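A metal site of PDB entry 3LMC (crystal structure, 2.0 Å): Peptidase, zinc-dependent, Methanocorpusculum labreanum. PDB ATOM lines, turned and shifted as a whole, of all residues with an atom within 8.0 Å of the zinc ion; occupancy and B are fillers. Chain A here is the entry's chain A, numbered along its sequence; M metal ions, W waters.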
ATOM      1  N   GLY A 109      17.910   4.700 -20.207  1.00  0.00           N
ATOM      2  CA  GLY A 109      16.792   4.422 -19.315  1.00  0.00           C
ATOM      3  C   GLY A 109      15.703   3.627 -19.992  1.00  0.00           C
ATOM      4  O   GLY A 109      15.802   3.341 -21.186  1.00  0.00           O
ATOM      5  N   LEU A 110      14.647   3.282 -19.253  1.00  0.00           N
ATOM      6  CA  LEU A 110      13.578   2.474 -19.812  1.00  0.00           C
ATOM      7  C   LEU A 110      12.360   2.591 -18.898  1.00  0.00           C
ATOM      8  O   LEU A 110      12.507   2.836 -17.703  1.00  0.00           O
ATOM      9  CB  LEU A 110      14.016   1.016 -19.905  1.00  0.00           C
ATOM     10  CG  LEU A 110      13.158   0.088 -20.741  1.00  0.00           C
ATOM     11  CD1 LEU A 110      13.209   0.533 -22.190  1.00  0.00           C
ATOM     12  CD2 LEU A 110      13.653  -1.330 -20.615  1.00  0.00           C
ATOM     13  N   ALA A 111      11.168   2.397 -19.458  1.00  0.00           N
ATOM     14  CA  ALA A 111       9.942   2.505 -18.667  1.00  0.00           C
ATOM     15  C   ALA A 111       9.069   1.297 -18.923  1.00  0.00           C
ATOM     16  O   ALA A 111       9.118   0.732 -20.025  1.00  0.00           O
ATOM     17  CB  ALA A 111       9.214   3.786 -19.015  1.00  0.00           C
ATOM     18  N   GLU A 146      16.392  12.739 -18.746  1.00  0.00           N
ATOM     19  CA  GLU A 146      16.097  11.369 -19.146  1.00  0.00           C
ATOM     20  C   GLU A 146      15.152  10.736 -18.122  1.00  0.00           C
ATOM     21  O   GLU A 146      14.332   9.887 -18.467  1.00  0.00           O
ATOM     22  CB  GLU A 146      17.380  10.543 -19.301  1.00  0.00           C
ATOM     23  CG  GLU A 146      17.145   9.051 -19.469  1.00  0.00           C
ATOM     24  CD  GLU A 146      16.547   8.687 -20.826  1.00  0.00           C
ATOM     25  OE1 GLU A 146      16.428   9.584 -21.688  1.00  0.00           O
ATOM     26  OE2 GLU A 146      16.220   7.503 -21.026  1.00  0.00           O
ATOM     27  N   HIS A 149      11.716  12.042 -18.936  1.00  0.00           N
ATOM     28  CA  HIS A 149      11.330  11.317 -20.149  1.00  0.00           C
ATOM     29  C   HIS A 149      10.680   9.979 -19.792  1.00  0.00           C
ATOM     30  O   HIS A 149       9.537   9.726 -20.149  1.00  0.00           O
ATOM     31  CB  HIS A 149      12.571  11.070 -21.016  1.00  0.00           C
ATOM     32  CG  HIS A 149      12.308  10.249 -22.223  1.00  0.00           C
ATOM     33  ND1 HIS A 149      12.105  10.805 -23.470  1.00  0.00           N
ATOM     34  CD2 HIS A 149      12.209   8.908 -22.391  1.00  0.00           C
ATOM     35  CE1 HIS A 149      11.879   9.841 -24.345  1.00  0.00           C
ATOM     36  NE2 HIS A 149      11.947   8.686 -23.721  1.00  0.00           N
ATOM     37  N   GLU A 150      11.412   9.135 -19.067  1.00  0.00           N
ATOM     38  CA  GLU A 150      10.914   7.842 -18.624  1.00  0.00           C
ATOM     39  C   GLU A 150       9.617   7.971 -17.841  1.00  0.00           C
ATOM     40  O   GLU A 150       8.702   7.193 -18.057  1.00  0.00           O
ATOM     41  CB  GLU A 150      11.949   7.113 -17.775  1.00  0.00           C
ATOM     42  CG  GLU A 150      13.315   6.931 -18.437  1.00  0.00           C
ATOM     43  CD  GLU A 150      13.222   6.303 -19.809  1.00  0.00           C
ATOM     44  OE1 GLU A 150      12.107   5.981 -20.272  1.00  0.00           O
ATOM     45  OE2 GLU A 150      14.277   6.127 -20.454  1.00  0.00           O
ATOM     46  N   HIS A 153       6.556   8.607 -19.966  1.00  0.00           N
ATOM     47  CA  HIS A 153       6.022   7.314 -20.448  1.00  0.00           C
ATOM     48  C   HIS A 153       5.055   6.663 -19.453  1.00  0.00           C
ATOM     49  O   HIS A 153       4.037   6.103 -19.827  1.00  0.00           O
ATOM     50  CB  HIS A 153       7.153   6.331 -20.689  1.00  0.00           C
ATOM     51  CG  HIS A 153       7.957   6.595 -21.909  1.00  0.00           C
ATOM     52  ND1 HIS A 153       7.389   6.902 -23.127  1.00  0.00           N
ATOM     53  CD2 HIS A 153       9.294   6.546 -22.119  1.00  0.00           C
ATOM     54  CE1 HIS A 153       8.344   7.053 -24.024  1.00  0.00           C
ATOM     55  NE2 HIS A 153       9.505   6.834 -23.439  1.00  0.00           N
ATOM     56  N   LEU A 157       2.584   9.152 -22.275  1.00  0.00           N
ATOM     57  CA  LEU A 157       3.181   9.879 -23.397  1.00  0.00           C
ATOM     58  C   LEU A 157       4.118   8.989 -24.197  1.00  0.00           C
ATOM     59  O   LEU A 157       4.853   8.167 -23.638  1.00  0.00           O
ATOM     60  CB  LEU A 157       3.918  11.119 -22.916  1.00  0.00           C
ATOM     61  CG  LEU A 157       3.092  12.348 -22.536  1.00  0.00           C
ATOM     62  CD1 LEU A 157       2.284  12.050 -21.285  1.00  0.00           C
ATOM     63  CD2 LEU A 157       4.008  13.531 -22.317  1.00  0.00           C
ATOM     64  N   GLY A 158       4.100   9.153 -25.522  1.00  0.00           N
ATOM     65  CA  GLY A 158       5.039   8.446 -26.369  1.00  0.00           C
ATOM     66  C   GLY A 158       6.198   9.349 -26.724  1.00  0.00           C
ATOM     67  O   GLY A 158       6.358  10.415 -26.128  1.00  0.00           O
ATOM     68  N   HIS A 159       7.005   8.955 -27.698  1.00  0.00           N
ATOM     69  CA  HIS A 159       8.117   9.804 -28.126  1.00  0.00           C
ATOM     70  C   HIS A 159       7.685  10.995 -28.953  1.00  0.00           C
ATOM     71  O   HIS A 159       6.831  10.882 -29.823  1.00  0.00           O
ATOM     72  CB  HIS A 159       9.153   8.999 -28.899  1.00  0.00           C
ATOM     73  CG  HIS A 159       9.966   8.092 -28.029  1.00  0.00           C
ATOM     74  ND1 HIS A 159      10.350   6.828 -28.428  1.00  0.00           N
ATOM     75  CD2 HIS A 159      10.429   8.260 -26.781  1.00  0.00           C
ATOM     76  CE1 HIS A 159      11.038   6.265 -27.453  1.00  0.00           C
ATOM     77  NE2 HIS A 159      11.106   7.118 -26.439  1.00  0.00           N
ATOM     78  N   CYS A 160       8.304  12.130 -28.670  1.00  0.00           N
ATOM     79  CA  CYS A 160       7.951  13.369 -29.326  1.00  0.00           C
ATOM     80  C   CYS A 160       8.967  13.692 -30.418  1.00  0.00           C
ATOM     81  O   CYS A 160      10.147  13.313 -30.315  1.00  0.00           O
ATOM     82  CB  CYS A 160       7.936  14.465 -28.264  1.00  0.00           C
ATOM     83  SG  CYS A 160       7.563  16.078 -28.870  1.00  0.00           S
ATOM     84  N   ILE A 166      11.328  17.112 -23.710  1.00  0.00           N
ATOM     85  CA  ILE A 166      11.765  16.053 -22.811  1.00  0.00           C
ATOM     86  C   ILE A 166      11.438  14.665 -23.367  1.00  0.00           C
ATOM     87  O   ILE A 166      12.170  13.694 -23.110  1.00  0.00           O
ATOM     88  CB  ILE A 166      11.098  16.175 -21.427  1.00  0.00           C
ATOM     89  CG1 ILE A 166      11.691  17.357 -20.660  1.00  0.00           C
ATOM     90  CG2 ILE A 166      11.290  14.883 -20.624  1.00  0.00           C
ATOM     91  CD1 ILE A 166      12.809  17.002 -19.752  1.00  0.00           C
ATOM     92  N   MET A 167      10.359  14.581 -24.145  1.00  0.00           N
ATOM     93  CA  MET A 167       9.859  13.302 -24.671  1.00  0.00           C
ATOM     94  C   MET A 167      10.551  12.835 -25.955  1.00  0.00           C
ATOM     95  O   MET A 167      10.253  11.754 -26.469  1.00  0.00           O
ATOM     96  CB  MET A 167       8.342  13.338 -24.908  1.00  0.00           C
ATOM     97  CG  MET A 167       7.489  13.315 -23.665  1.00  0.00           C
ATOM     98  SD  MET A 167       8.136  12.084 -22.245  1.00  0.00           S
ATOM     99  CE  MET A 167       7.003  12.779 -20.832  1.00  0.00           C
ATOM    100  N   TYR A 168      11.463  13.644 -26.478  1.00  0.00           N
ATOM    101  CA  TYR A 168      12.247  13.247 -27.631  1.00  0.00           C
ATOM    102  C   TYR A 168      13.162  12.088 -27.226  1.00  0.00           C
ATOM    103  O   TYR A 168      13.668  12.059 -26.105  1.00  0.00           O
ATOM    104  CB  TYR A 168      13.085  14.424 -28.104  1.00  0.00           C
ATOM    105  CG  TYR A 168      13.982  14.106 -29.281  1.00  0.00           C
ATOM    106  CD1 TYR A 168      15.353  13.956 -29.108  1.00  0.00           C
ATOM    107  CD2 TYR A 168      13.470  13.966 -30.561  1.00  0.00           C
ATOM    108  CE1 TYR A 168      16.177  13.653 -30.170  1.00  0.00           C
ATOM    109  CE2 TYR A 168      14.282  13.671 -31.624  1.00  0.00           C
ATOM    110  CZ  TYR A 168      15.640  13.515 -31.430  1.00  0.00           C
ATOM    111  OH  TYR A 168      16.465  13.226 -32.489  1.00  0.00           O
ATOM    112  N   CYS A 169      13.366  11.128 -28.119  1.00  0.00           N
ATOM    113  CA  CYS A 169      14.225   9.991 -27.811  1.00  0.00           C
ATOM    114  C   CYS A 169      15.622  10.242 -28.366  1.00  0.00           C
ATOM    115  O   CYS A 169      15.805  10.270 -29.589  1.00  0.00           O
ATOM    116  CB  CYS A 169      13.649   8.688 -28.367  1.00  0.00           C
ATOM    117  SG  CYS A 169      14.553   7.193 -27.819  1.00  0.00           S
ATOM    118  N   PRO A 170      16.617  10.425 -27.479  1.00  0.00           N
ATOM    119  CA  PRO A 170      17.997  10.747 -27.851  1.00  0.00           C
ATOM    120  C   PRO A 170      18.747   9.537 -28.402  1.00  0.00           C
ATOM    121  O   PRO A 170      18.744   8.491 -27.761  1.00  0.00           O
ATOM    122  CB  PRO A 170      18.648  11.152 -26.511  1.00  0.00           C
ATOM    123  CG  PRO A 170      17.548  11.098 -25.469  1.00  0.00           C
ATOM    124  CD  PRO A 170      16.463  10.231 -26.026  1.00  0.00           C
ATOM    125  N   LYS A 179      18.386  18.415 -25.635  1.00  0.00           N
ATOM    126  CA  LYS A 179      17.031  18.478 -25.081  1.00  0.00           C
ATOM    127  C   LYS A 179      17.012  19.569 -24.028  1.00  0.00           C
ATOM    128  O   LYS A 179      18.036  19.852 -23.405  1.00  0.00           O
ATOM    129  CB  LYS A 179      16.604  17.148 -24.480  1.00  0.00           C
ATOM    130  CG  LYS A 179      16.580  16.005 -25.467  1.00  0.00           C
ATOM    131  CD  LYS A 179      16.407  14.692 -24.731  1.00  0.00           C
ATOM    132  CE  LYS A 179      14.997  14.536 -24.208  1.00  0.00           C
ATOM    133  NZ  LYS A 179      14.889  13.291 -23.378  1.00  0.00           N
HETATM  134 ZN    ZN M   1      11.503   6.635 -24.364  1.00  0.00          ZN
HETATM  135  O   HOH W   1      10.089   3.830 -24.610  1.00  0.00           O
HETATM  136  O   HOH W   2      12.559   5.025 -22.981  1.00  0.00           O
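NE2 of His 159 sits close to SG of Cys 169.
ND1 of His 149 is in hydrogen-bond range of O of Tyr 168 (3.3 Å).
O of Ile 166 sits at hydrogen-bond distance from ND1 of His 149, at 2.9 Å.
ND1 of His 153 sits at hydrogen-bond distance from O of Leu 157 (2.9 Å).
The zinc ion is bound by NE2 of His 159 (2.2 Å).
The zinc ion is bound by NE2 of His 149.
The zinc ion is bound by a ring nitrogen (NE2) of His 153 (2.2 Å).
Water W2 is bound to the zinc ion (2.4 Å).
The zinc ion has four donor atoms within binding distance.
Within 4 Å of the zinc ion: His 149, His 153 and His 159.
The nearest printed residue that does not touch the zinc ion is Glu 150 (4.2 Å).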
